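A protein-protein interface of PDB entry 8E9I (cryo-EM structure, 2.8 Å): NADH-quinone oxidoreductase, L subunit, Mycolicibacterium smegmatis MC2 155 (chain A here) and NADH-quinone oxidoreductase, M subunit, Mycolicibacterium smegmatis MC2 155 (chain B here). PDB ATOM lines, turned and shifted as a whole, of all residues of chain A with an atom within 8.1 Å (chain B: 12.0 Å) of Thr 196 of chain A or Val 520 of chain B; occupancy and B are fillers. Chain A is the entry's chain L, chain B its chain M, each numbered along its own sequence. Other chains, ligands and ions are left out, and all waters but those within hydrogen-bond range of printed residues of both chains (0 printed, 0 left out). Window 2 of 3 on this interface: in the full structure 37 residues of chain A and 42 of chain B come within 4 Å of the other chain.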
ATOM      1  N   ALA A 189      22.253  -4.235  19.091  1.00  0.00           N
ATOM      2  CA  ALA A 189      21.426  -3.082  19.426  1.00  0.00           C
ATOM      3  C   ALA A 189      20.256  -2.951  18.459  1.00  0.00           C
ATOM      4  O   ALA A 189      19.108  -2.768  18.881  1.00  0.00           O
ATOM      5  CB  ALA A 189      22.275  -1.813  19.424  1.00  0.00           C
ATOM      6  N   LEU A 190      20.528  -3.056  17.157  1.00  0.00           N
ATOM      7  CA  LEU A 190      19.458  -2.955  16.171  1.00  0.00           C
ATOM      8  C   LEU A 190      18.455  -4.090  16.318  1.00  0.00           C
ATOM      9  O   LEU A 190      17.246  -3.882  16.169  1.00  0.00           O
ATOM     10  CB  LEU A 190      20.031  -2.942  14.755  1.00  0.00           C
ATOM     11  CG  LEU A 190      20.381  -1.558  14.212  1.00  0.00           C
ATOM     12  CD1 LEU A 190      21.630  -1.016  14.885  1.00  0.00           C
ATOM     13  CD2 LEU A 190      20.558  -1.607  12.708  1.00  0.00           C
ATOM     14  N   MET A 191      18.936  -5.305  16.580  1.00  0.00           N
ATOM     15  CA  MET A 191      18.015  -6.422  16.752  1.00  0.00           C
ATOM     16  C   MET A 191      17.076  -6.166  17.921  1.00  0.00           C
ATOM     17  O   MET A 191      15.869  -6.412  17.822  1.00  0.00           O
ATOM     18  CB  MET A 191      18.792  -7.721  16.958  1.00  0.00           C
ATOM     19  N   ILE A 192      17.610  -5.663  19.033  1.00  0.00           N
ATOM     20  CA  ILE A 192      16.763  -5.334  20.175  1.00  0.00           C
ATOM     21  C   ILE A 192      15.761  -4.257  19.792  1.00  0.00           C
ATOM     22  O   ILE A 192      14.569  -4.346  20.109  1.00  0.00           O
ATOM     23  CB  ILE A 192      17.624  -4.892  21.369  1.00  0.00           C
ATOM     24  CG1 ILE A 192      18.518  -6.038  21.823  1.00  0.00           C
ATOM     25  CG2 ILE A 192      16.740  -4.436  22.514  1.00  0.00           C
ATOM     26  CD1 ILE A 192      19.722  -5.582  22.570  1.00  0.00           C
ATOM     27  N   MET A 193      16.232  -3.219  19.103  1.00  0.00           N
ATOM     28  CA  MET A 193      15.342  -2.133  18.717  1.00  0.00           C
ATOM     29  C   MET A 193      14.179  -2.657  17.891  1.00  0.00           C
ATOM     30  O   MET A 193      13.020  -2.311  18.137  1.00  0.00           O
ATOM     31  CB  MET A 193      16.120  -1.074  17.938  1.00  0.00           C
ATOM     32  CG  MET A 193      16.903  -0.122  18.822  1.00  0.00           C
ATOM     33  SD  MET A 193      17.581   1.281  17.919  1.00  0.00           S
ATOM     34  CE  MET A 193      19.237   0.693  17.599  1.00  0.00           C
ATOM     35  N   PHE A 194      14.468  -3.513  16.915  1.00  0.00           N
ATOM     36  CA  PHE A 194      13.413  -4.023  16.047  1.00  0.00           C
ATOM     37  C   PHE A 194      12.474  -4.948  16.807  1.00  0.00           C
ATOM     38  O   PHE A 194      11.249  -4.829  16.702  1.00  0.00           O
ATOM     39  CB  PHE A 194      14.022  -4.751  14.855  1.00  0.00           C
ATOM     40  CG  PHE A 194      13.007  -5.394  13.961  1.00  0.00           C
ATOM     41  CD1 PHE A 194      12.300  -4.644  13.041  1.00  0.00           C
ATOM     42  CD2 PHE A 194      12.753  -6.751  14.050  1.00  0.00           C
ATOM     43  CE1 PHE A 194      11.369  -5.235  12.222  1.00  0.00           C
ATOM     44  CE2 PHE A 194      11.824  -7.348  13.232  1.00  0.00           C
ATOM     45  CZ  PHE A 194      11.129  -6.589  12.319  1.00  0.00           C
ATOM     46  N   ALA A 195      13.033  -5.886  17.575  1.00  0.00           N
ATOM     47  CA  ALA A 195      12.205  -6.863  18.271  1.00  0.00           C
ATOM     48  C   ALA A 195      11.320  -6.206  19.316  1.00  0.00           C
ATOM     49  O   ALA A 195      10.263  -6.744  19.661  1.00  0.00           O
ATOM     50  CB  ALA A 195      13.085  -7.926  18.927  1.00  0.00           C
ATOM     51  N   THR A 196      11.731  -5.053  19.835  1.00  0.00           N
ATOM     52  CA  THR A 196      10.970  -4.400  20.888  1.00  0.00           C
ATOM     53  C   THR A 196      10.027  -3.334  20.346  1.00  0.00           C
ATOM     54  O   THR A 196       8.951  -3.115  20.912  1.00  0.00           O
ATOM     55  CB  THR A 196      11.934  -3.790  21.901  1.00  0.00           C
ATOM     56  OG1 THR A 196      12.810  -2.874  21.234  1.00  0.00           O
ATOM     57  CG2 THR A 196      12.759  -4.889  22.551  1.00  0.00           C
ATOM     58  N   ILE A 197      10.406  -2.673  19.258  1.00  0.00           N
ATOM     59  CA  ILE A 197       9.590  -1.635  18.647  1.00  0.00           C
ATOM     60  C   ILE A 197       9.018  -2.085  17.309  1.00  0.00           C
ATOM     61  O   ILE A 197       7.874  -1.773  16.985  1.00  0.00           O
ATOM     62  CB  ILE A 197      10.416  -0.344  18.478  1.00  0.00           C
ATOM     63  CG1 ILE A 197      10.925   0.151  19.832  1.00  0.00           C
ATOM     64  CG2 ILE A 197       9.586   0.727  17.801  1.00  0.00           C
ATOM     65  CD1 ILE A 197      12.061   1.143  19.722  1.00  0.00           C
ATOM     66  N   GLY A 198       9.802  -2.819  16.527  1.00  0.00           N
ATOM     67  CA  GLY A 198       9.409  -3.128  15.170  1.00  0.00           C
ATOM     68  C   GLY A 198       9.712  -2.033  14.179  1.00  0.00           C
ATOM     69  O   GLY A 198       9.232  -2.088  13.043  1.00  0.00           O
ATOM     70  N   SER A 199      10.490  -1.030  14.575  1.00  0.00           N
ATOM     71  CA  SER A 199      10.899   0.028  13.668  1.00  0.00           C
ATOM     72  C   SER A 199      12.389   0.262  13.838  1.00  0.00           C
ATOM     73  O   SER A 199      12.955   0.030  14.908  1.00  0.00           O
ATOM     74  CB  SER A 199      10.130   1.326  13.922  1.00  0.00           C
ATOM     75  OG  SER A 199      10.448   2.294  12.935  1.00  0.00           O
ATOM     76  N   VAL A 205      11.787   4.779  16.273  1.00  0.00           N
ATOM     77  CA  VAL A 205      12.456   4.289  17.474  1.00  0.00           C
ATOM     78  C   VAL A 205      12.356   5.318  18.590  1.00  0.00           C
ATOM     79  O   VAL A 205      12.040   4.989  19.738  1.00  0.00           O
ATOM     80  CB  VAL A 205      13.922   3.937  17.166  1.00  0.00           C
ATOM     81  N   ALA A 207      10.164   7.666  18.866  1.00  0.00           N
ATOM     82  CA  ALA A 207       8.779   7.842  19.284  1.00  0.00           C
ATOM     83  C   ALA A 207       8.321   6.715  20.199  1.00  0.00           C
ATOM     84  O   ALA A 207       7.530   6.951  21.118  1.00  0.00           O
ATOM     85  CB  ALA A 207       7.872   7.932  18.059  1.00  0.00           C
ATOM     86  N   ALA A 208       8.789   5.493  19.965  1.00  0.00           N
ATOM     87  CA  ALA A 208       8.410   4.368  20.809  1.00  0.00           C
ATOM     88  C   ALA A 208       9.255   4.255  22.068  1.00  0.00           C
ATOM     89  O   ALA A 208       8.858   3.548  23.002  1.00  0.00           O
ATOM     90  CB  ALA A 208       8.513   3.057  20.027  1.00  0.00           C
ATOM     91  N   ALA A 209      10.397   4.936  22.119  1.00  0.00           N
ATOM     92  CA  ALA A 209      11.289   4.815  23.267  1.00  0.00           C
ATOM     93  C   ALA A 209      10.608   5.068  24.605  1.00  0.00           C
ATOM     94  O   ALA A 209      10.886   4.319  25.556  1.00  0.00           O
ATOM     95  CB  ALA A 209      12.475   5.772  23.088  1.00  0.00           C
ATOM     96  N   PRO A 210       9.740   6.069  24.764  1.00  0.00           N
ATOM     97  CA  PRO A 210       9.179   6.334  26.098  1.00  0.00           C
ATOM     98  C   PRO A 210       8.474   5.137  26.711  1.00  0.00           C
ATOM     99  O   PRO A 210       8.518   4.976  27.937  1.00  0.00           O
ATOM    100  CB  PRO A 210       8.208   7.494  25.845  1.00  0.00           C
ATOM    101  CG  PRO A 210       8.722   8.152  24.614  1.00  0.00           C
ATOM    102  CD  PRO A 210       9.255   7.038  23.768  1.00  0.00           C
ATOM    103  N   GLY A 211       7.836   4.288  25.908  1.00  0.00           N
ATOM    104  CA  GLY A 211       7.187   3.106  26.438  1.00  0.00           C
ATOM    105  C   GLY A 211       8.120   1.970  26.791  1.00  0.00           C
ATOM    106  O   GLY A 211       7.686   1.001  27.420  1.00  0.00           O
ATOM    107  N   LEU A 212       9.390   2.070  26.412  1.00  0.00           N
ATOM    108  CA  LEU A 212      10.354   1.015  26.675  1.00  0.00           C
ATOM    109  C   LEU A 212      10.722   0.981  28.154  1.00  0.00           C
ATOM    110  O   LEU A 212      10.811   2.012  28.825  1.00  0.00           O
ATOM    111  CB  LEU A 212      11.612   1.212  25.828  1.00  0.00           C
ATOM    112  N   SER A 213      10.940  -0.228  28.658  1.00  0.00           N
ATOM    113  CA  SER A 213      11.349  -0.391  30.040  1.00  0.00           C
ATOM    114  C   SER A 213      12.815  -0.012  30.209  1.00  0.00           C
ATOM    115  O   SER A 213      13.574   0.103  29.243  1.00  0.00           O
ATOM    116  CB  SER A 213      11.130  -1.827  30.499  1.00  0.00           C
ATOM    117  OG  SER A 213      12.017  -2.701  29.830  1.00  0.00           O
ATOM    118  N   ALA A 215      15.151  -1.796  31.304  1.00  0.00           N
ATOM    119  CA  ALA A 215      16.061  -2.872  30.926  1.00  0.00           C
ATOM    120  C   ALA A 215      16.322  -2.872  29.424  1.00  0.00           C
ATOM    121  O   ALA A 215      17.471  -2.987  28.979  1.00  0.00           O
ATOM    122  CB  ALA A 215      15.493  -4.218  31.376  1.00  0.00           C
ATOM    123  N   THR A 216      15.263  -2.754  28.623  1.00  0.00           N
ATOM    124  CA  THR A 216      15.436  -2.725  27.176  1.00  0.00           C
ATOM    125  C   THR A 216      16.263  -1.518  26.757  1.00  0.00           C
ATOM    126  O   THR A 216      17.184  -1.627  25.935  1.00  0.00           O
ATOM    127  CB  THR A 216      14.070  -2.704  26.489  1.00  0.00           C
ATOM    128  OG1 THR A 216      13.356  -3.906  26.800  1.00  0.00           O
ATOM    129  CG2 THR A 216      14.224  -2.597  24.991  1.00  0.00           C
ATOM    130  N   LEU A 217      15.945  -0.352  27.319  1.00  0.00           N
ATOM    131  CA  LEU A 217      16.709   0.844  27.002  1.00  0.00           C
ATOM    132  C   LEU A 217      18.154   0.703  27.443  1.00  0.00           C
ATOM    133  O   LEU A 217      19.065   1.130  26.729  1.00  0.00           O
ATOM    134  CB  LEU A 217      16.059   2.062  27.657  1.00  0.00           C
ATOM    135  CG  LEU A 217      14.697   2.441  27.076  1.00  0.00           C
ATOM    136  CD1 LEU A 217      13.810   3.094  28.124  1.00  0.00           C
ATOM    137  CD2 LEU A 217      14.887   3.361  25.885  1.00  0.00           C
ATOM    138  N   ALA A 219      19.900  -2.057  27.656  1.00  0.00           N
ATOM    139  CA  ALA A 219      20.572  -2.945  26.716  1.00  0.00           C
ATOM    140  C   ALA A 219      20.916  -2.210  25.428  1.00  0.00           C
ATOM    141  O   ALA A 219      22.055  -2.273  24.946  1.00  0.00           O
ATOM    142  CB  ALA A 219      19.693  -4.159  26.425  1.00  0.00           C
ATOM    143  N   ILE A 220      19.944  -1.495  24.860  1.00  0.00           N
ATOM    144  CA  ILE A 220      20.188  -0.807  23.595  1.00  0.00           C
ATOM    145  C   ILE A 220      21.302   0.219  23.762  1.00  0.00           C
ATOM    146  O   ILE A 220      22.246   0.279  22.963  1.00  0.00           O
ATOM    147  CB  ILE A 220      18.897  -0.153  23.074  1.00  0.00           C
ATOM    148  CG1 ILE A 220      17.858  -1.221  22.731  1.00  0.00           C
ATOM    149  CG2 ILE A 220      19.195   0.701  21.851  1.00  0.00           C
ATOM    150  CD1 ILE A 220      16.467  -0.666  22.525  1.00  0.00           C
ATOM    151  N   THR B 343      10.148 -16.838  10.544  1.00  0.00           N
ATOM    152  CA  THR B 343       9.825 -15.422  10.616  1.00  0.00           C
ATOM    153  C   THR B 343       9.991 -14.814   9.236  1.00  0.00           C
ATOM    154  O   THR B 343      10.985 -15.078   8.554  1.00  0.00           O
ATOM    155  CB  THR B 343      10.727 -14.691  11.613  1.00  0.00           C
ATOM    156  OG1 THR B 343      10.679 -15.359  12.879  1.00  0.00           O
ATOM    157  CG2 THR B 343      10.281 -13.250  11.783  1.00  0.00           C
ATOM    158  N   GLN B 345      10.863 -11.925   8.192  1.00  0.00           N
ATOM    159  CA  GLN B 345      12.219 -11.405   8.096  1.00  0.00           C
ATOM    160  C   GLN B 345      13.215 -12.542   7.941  1.00  0.00           C
ATOM    161  O   GLN B 345      14.050 -12.518   7.037  1.00  0.00           O
ATOM    162  CB  GLN B 345      12.554 -10.563   9.325  1.00  0.00           C
ATOM    163  CG  GLN B 345      11.824  -9.236   9.394  1.00  0.00           C
ATOM    164  CD  GLN B 345      10.388  -9.384   9.837  1.00  0.00           C
ATOM    165  OE1 GLN B 345      10.046 -10.320  10.559  1.00  0.00           O
ATOM    166  NE2 GLN B 345       9.539  -8.460   9.412  1.00  0.00           N
ATOM    167  N   PHE B 417      21.895  -9.707   8.011  1.00  0.00           N
ATOM    168  CA  PHE B 417      21.114  -8.819   8.857  1.00  0.00           C
ATOM    169  C   PHE B 417      19.681  -9.314   8.977  1.00  0.00           C
ATOM    170  O   PHE B 417      19.208  -9.635  10.074  1.00  0.00           O
ATOM    171  CB  PHE B 417      21.157  -7.407   8.284  1.00  0.00           C
ATOM    172  CG  PHE B 417      20.245  -6.451   8.973  1.00  0.00           C
ATOM    173  CD1 PHE B 417      20.550  -5.971  10.230  1.00  0.00           C
ATOM    174  CD2 PHE B 417      19.077  -6.032   8.365  1.00  0.00           C
ATOM    175  CE1 PHE B 417      19.714  -5.092  10.866  1.00  0.00           C
ATOM    176  CE2 PHE B 417      18.236  -5.151   8.997  1.00  0.00           C
ATOM    177  CZ  PHE B 417      18.554  -4.681  10.249  1.00  0.00           C
ATOM    178  N   LEU B 420      19.515 -12.420  10.986  1.00  0.00           N
ATOM    179  CA  LEU B 420      19.780 -12.165  12.397  1.00  0.00           C
ATOM    180  C   LEU B 420      18.591 -11.478  13.047  1.00  0.00           C
ATOM    181  O   LEU B 420      18.098 -11.918  14.092  1.00  0.00           O
ATOM    182  CB  LEU B 420      21.040 -11.317  12.561  1.00  0.00           C
ATOM    183  CG  LEU B 420      22.377 -12.052  12.499  1.00  0.00           C
ATOM    184  CD1 LEU B 420      23.523 -11.063  12.626  1.00  0.00           C
ATOM    185  CD2 LEU B 420      22.471 -13.115  13.578  1.00  0.00           C
ATOM    186  N   ILE B 421      18.098 -10.407  12.425  1.00  0.00           N
ATOM    187  CA  ILE B 421      16.905  -9.742  12.935  1.00  0.00           C
ATOM    188  C   ILE B 421      15.812 -10.769  13.178  1.00  0.00           C
ATOM    189  O   ILE B 421      15.229 -10.846  14.266  1.00  0.00           O
ATOM    190  CB  ILE B 421      16.442  -8.651  11.954  1.00  0.00           C
ATOM    191  CG1 ILE B 421      17.463  -7.514  11.889  1.00  0.00           C
ATOM    192  CG2 ILE B 421      15.092  -8.115  12.364  1.00  0.00           C
ATOM    193  CD1 ILE B 421      17.376  -6.541  13.043  1.00  0.00           C
ATOM    194  N   GLY B 422      15.555 -11.614  12.178  1.00  0.00           N
ATOM    195  CA  GLY B 422      14.515 -12.614  12.328  1.00  0.00           C
ATOM    196  C   GLY B 422      14.758 -13.516  13.519  1.00  0.00           C
ATOM    197  O   GLY B 422      13.833 -13.836  14.269  1.00  0.00           O
ATOM    198  N   THR B 423      16.010 -13.924  13.722  1.00  0.00           N
ATOM    199  CA  THR B 423      16.314 -14.826  14.825  1.00  0.00           C
ATOM    200  C   THR B 423      16.096 -14.143  16.167  1.00  0.00           C
ATOM    201  O   THR B 423      15.807 -14.805  17.168  1.00  0.00           O
ATOM    202  CB  THR B 423      17.750 -15.331  14.713  1.00  0.00           C
ATOM    203  N   PHE B 424      16.232 -12.817  16.213  1.00  0.00           N
ATOM    204  CA  PHE B 424      16.152 -12.144  17.502  1.00  0.00           C
ATOM    205  C   PHE B 424      14.727 -12.115  18.030  1.00  0.00           C
ATOM    206  O   PHE B 424      14.517 -12.108  19.246  1.00  0.00           O
ATOM    207  CB  PHE B 424      16.701 -10.725  17.400  1.00  0.00           C
ATOM    208  CG  PHE B 424      17.184 -10.183  18.707  1.00  0.00           C
ATOM    209  CD1 PHE B 424      16.304  -9.609  19.604  1.00  0.00           C
ATOM    210  CD2 PHE B 424      18.520 -10.263  19.048  1.00  0.00           C
ATOM    211  CE1 PHE B 424      16.752  -9.119  20.811  1.00  0.00           C
ATOM    212  CE2 PHE B 424      18.970  -9.774  20.251  1.00  0.00           C
ATOM    213  CZ  PHE B 424      18.086  -9.203  21.136  1.00  0.00           C
ATOM    214  N   THR B 425      13.738 -12.096  17.137  1.00  0.00           N
ATOM    215  CA  THR B 425      12.355 -11.969  17.579  1.00  0.00           C
ATOM    216  C   THR B 425      11.831 -13.265  18.179  1.00  0.00           C
ATOM    217  O   THR B 425      10.740 -13.278  18.760  1.00  0.00           O
ATOM    218  CB  THR B 425      11.464 -11.542  16.416  1.00  0.00           C
ATOM    219  OG1 THR B 425      11.317 -12.633  15.503  1.00  0.00           O
ATOM    220  CG2 THR B 425      12.061 -10.350  15.691  1.00  0.00           C
ATOM    221  N   ARG B 426      12.571 -14.362  18.038  1.00  0.00           N
ATOM    222  CA  ARG B 426      12.151 -15.657  18.561  1.00  0.00           C
ATOM    223  C   ARG B 426      13.208 -16.355  19.399  1.00  0.00           C
ATOM    224  O   ARG B 426      12.864 -17.176  20.248  1.00  0.00           O
ATOM    225  CB  ARG B 426      11.743 -16.576  17.408  1.00  0.00           C
ATOM    226  CG  ARG B 426      10.428 -16.191  16.768  1.00  0.00           C
ATOM    227  CD  ARG B 426       9.841 -17.332  15.969  1.00  0.00           C
ATOM    228  NE  ARG B 426       8.385 -17.296  15.963  1.00  0.00           N
ATOM    229  CZ  ARG B 426       7.652 -16.705  15.030  1.00  0.00           C
ATOM    230  NH1 ARG B 426       8.207 -16.054  14.023  1.00  0.00           N
ATOM    231  NH2 ARG B 426       6.326 -16.767  15.111  1.00  0.00           N
ATOM    232  N   TYR B 427      14.488 -16.076  19.175  1.00  0.00           N
ATOM    233  CA  TYR B 427      15.573 -16.735  19.903  1.00  0.00           C
ATOM    234  C   TYR B 427      16.734 -15.765  20.031  1.00  0.00           C
ATOM    235  O   TYR B 427      17.765 -15.908  19.362  1.00  0.00           O
ATOM    236  CB  TYR B 427      16.000 -18.021  19.196  1.00  0.00           C
ATOM    237  CG  TYR B 427      14.870 -19.007  19.054  1.00  0.00           C
ATOM    238  CD1 TYR B 427      14.485 -19.807  20.121  1.00  0.00           C
ATOM    239  CD2 TYR B 427      14.170 -19.120  17.866  1.00  0.00           C
ATOM    240  CE1 TYR B 427      13.445 -20.704  20.002  1.00  0.00           C
ATOM    241  CE2 TYR B 427      13.129 -20.011  17.737  1.00  0.00           C
ATOM    242  CZ  TYR B 427      12.771 -20.802  18.810  1.00  0.00           C
ATOM    243  OH  TYR B 427      11.733 -21.694  18.686  1.00  0.00           O
ATOM    244  N   PRO B 428      16.603 -14.755  20.890  1.00  0.00           N
ATOM    245  CA  PRO B 428      17.657 -13.730  20.962  1.00  0.00           C
ATOM    246  C   PRO B 428      19.024 -14.293  21.304  1.00  0.00           C
ATOM    247  O   PRO B 428      20.037 -13.817  20.776  1.00  0.00           O
ATOM    248  CB  PRO B 428      17.140 -12.776  22.049  1.00  0.00           C
ATOM    249  CG  PRO B 428      16.187 -13.591  22.852  1.00  0.00           C
ATOM    250  CD  PRO B 428      15.543 -14.530  21.885  1.00  0.00           C
ATOM    251  N   ALA B 431      20.414 -15.542  18.266  1.00  0.00           N
ATOM    252  CA  ALA B 431      20.742 -14.433  17.380  1.00  0.00           C
ATOM    253  C   ALA B 431      22.100 -13.845  17.726  1.00  0.00           C
ATOM    254  O   ALA B 431      22.913 -13.583  16.836  1.00  0.00           O
ATOM    255  CB  ALA B 431      19.656 -13.363  17.453  1.00  0.00           C
ATOM    256  N   ASP B 515       5.115 -13.437  11.933  1.00  0.00           N
ATOM    257  CA  ASP B 515       6.158 -12.668  12.587  1.00  0.00           C
ATOM    258  C   ASP B 515       5.631 -12.152  13.922  1.00  0.00           C
ATOM    259  O   ASP B 515       4.556 -11.539  13.960  1.00  0.00           O
ATOM    260  CB  ASP B 515       6.603 -11.503  11.705  1.00  0.00           C
ATOM    261  N   PRO B 516       6.341 -12.371  15.024  1.00  0.00           N
ATOM    262  CA  PRO B 516       5.793 -11.995  16.328  1.00  0.00           C
ATOM    263  C   PRO B 516       5.588 -10.494  16.426  1.00  0.00           C
ATOM    264  O   PRO B 516       6.340  -9.701  15.857  1.00  0.00           O
ATOM    265  CB  PRO B 516       6.861 -12.479  17.310  1.00  0.00           C
ATOM    266  CG  PRO B 516       8.120 -12.372  16.542  1.00  0.00           C
ATOM    267  CD  PRO B 516       7.771 -12.711  15.117  1.00  0.00           C
ATOM    268  N   GLU B 517       4.548 -10.109  17.158  1.00  0.00           N
ATOM    269  CA  GLU B 517       4.224  -8.700  17.282  1.00  0.00           C
ATOM    270  C   GLU B 517       5.303  -7.984  18.095  1.00  0.00           C
ATOM    271  O   GLU B 517       5.909  -8.575  18.992  1.00  0.00           O
ATOM    272  CB  GLU B 517       2.861  -8.521  17.947  1.00  0.00           C
ATOM    273  N   PRO B 518       5.558  -6.710  17.807  1.00  0.00           N
ATOM    274  CA  PRO B 518       6.564  -5.977  18.582  1.00  0.00           C
ATOM    275  C   PRO B 518       6.164  -5.876  20.043  1.00  0.00           C
ATOM    276  O   PRO B 518       4.980  -5.874  20.384  1.00  0.00           O
ATOM    277  CB  PRO B 518       6.601  -4.603  17.908  1.00  0.00           C
ATOM    278  CG  PRO B 518       5.287  -4.473  17.240  1.00  0.00           C
ATOM    279  CD  PRO B 518       4.909  -5.851  16.805  1.00  0.00           C
ATOM    280  N   THR B 519       7.170  -5.799  20.910  1.00  0.00           N
ATOM    281  CA  THR B 519       6.939  -5.722  22.346  1.00  0.00           C
ATOM    282  C   THR B 519       6.029  -4.549  22.690  1.00  0.00           C
ATOM    283  O   THR B 519       5.040  -4.713  23.410  1.00  0.00           O
ATOM    284  CB  THR B 519       8.268  -5.593  23.090  1.00  0.00           C
ATOM    285  N   VAL B 520       6.352  -3.367  22.179  1.00  0.00           N
ATOM    286  CA  VAL B 520       5.545  -2.172  22.417  1.00  0.00           C
ATOM    287  C   VAL B 520       4.175  -2.379  21.784  1.00  0.00           C
ATOM    288  O   VAL B 520       4.072  -3.026  20.732  1.00  0.00           O
ATOM    289  CB  VAL B 520       6.231  -0.917  21.855  1.00  0.00           C
ATOM    290  N   PRO B 521       3.095  -1.857  22.382  1.00  0.00           N
ATOM    291  CA  PRO B 521       1.793  -2.080  21.748  1.00  0.00           C
ATOM    292  C   PRO B 521       1.606  -1.248  20.487  1.00  0.00           C
ATOM    293  O   PRO B 521       2.558  -1.113  19.718  1.00  0.00           O
ATOM    294  CB  PRO B 521       0.801  -1.664  22.834  1.00  0.00           C
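Of the 20 printed residues of chain B, 7 touch a printed residue of chain A.
Hydrophobic or aromatic side chains of chain B within 4 Å of the printed part of chain A: Ile 421, Phe 424, Pro 518 and Val 520.
Hydrophobic or aromatic side chains of chain A that line the printed part of chain B: Met 191, Ile 192, Phe 194 and Ala 195.
Among the printed residues, 13 pairs touch across the chains.
Among the printed residues, merely in contact across the chains: Met 191 of chain A with Ile 421 of chain B (3.8 Å), Met 191 of chain A with Phe 424 of chain B (3.3 Å), Ile 192 of chain A with Phe 424 of chain B (3.3 Å), Phe 194 of chain A with Gln 345 of chain B (3.8 Å), Phe 194 of chain A with Ile 421 of chain B (3.2 Å), Phe 194 of chain A with Thr 425 of chain B (3.9 Å), Ala 195 of chain A with Phe 424 of chain B (3.7 Å), Ala 195 of chain A with Pro 518 of chain B (3.9 Å), Ile 197 of chain A with Pro 518 of chain B (3.2 Å) and Gly 198 of chain A with Pro 518 of chain B (3.9 Å).
O of Ile 192 of chain A lies within hydrogen-bond range of OG1 of Thr 196 of chain A (2.6 Å).
The backbone carbonyl oxygen of Met 193 of chain A sits at hydrogen-bond distance from the side-chain hydroxyl of Thr 196 of chain A (3.2 Å).
O of Gly 422 of chain B sits at hydrogen-bond distance from OG1 of Thr 425 of chain B.
O of Ala 195 of chain A sits at hydrogen-bond distance from N of Thr 519 of chain B (3.5 Å).
The backbone carbonyl oxygen (O) of Thr 196 of chain A sits at hydrogen-bond distance from the backbone NH (N) of Thr 519 of chain B, at 3.2 Å.
O of Thr 196 of chain A lies within hydrogen-bond range of N of Val 520 of chain B (2.9 Å).
Ile 192 of chain A touches just one residue of chain B: Phe 424 (3.3 Å).
Of chain B, only Gln 345 (3.8 Å), Ile 421 (3.2 Å) and Thr 425 (3.9 Å) come within 4 Å of Phe 194 of chain A.
Ala 195 of chain A touches just these residues of chain B: Phe 424 (3.7 Å), Pro 518 (3.9 Å) and Thr 519 (3.5 Å).
Printed residues of chain B within 4 Å of Ile 197 of chain A: Pro 518.
Gly 198 of chain A touches one residue of chain B.
No residue of chain B comes within 4 Å of Ala 208 of chain A.
No residue of chain B comes within 4 Å of Gly 211 of chain A.
No residue of chain B comes within 4 Å of Thr 216 of chain A.
Of chain A, only Ala 195 (3.5 Å) and Thr 196 (3.2 Å) come within 4 Å of Thr 519 of chain B.
No residue of chain A comes within 4 Å of Pro 521 of chain B.
Printed residues of chain B within 4 Å of Met 191 of chain A: Ile 421 and Phe 424.
Printed residues of chain A within 4 Å of Pro 518 of chain B: Ala 195 (3.9 Å), Ile 197 (3.2 Å) and Gly 198 (3.9 Å).
Of the printed residues of chain A, Phe 424 of chain B touches Met 191 (3.3 Å), Ile 192 (3.3 Å) and Ala 195 (3.7 Å).
Printed residues of chain A within 4 Å of Ile 421 of chain B: Met 191 and Phe 194.
The nearest residue of chain A that does not touch Val 520 of chain B is Ile 197 of chain A (4.7 Å).
The nearest printed residue of chain A that does not touch Phe 424 of chain B is Thr 196 of chain A (6.1 Å).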
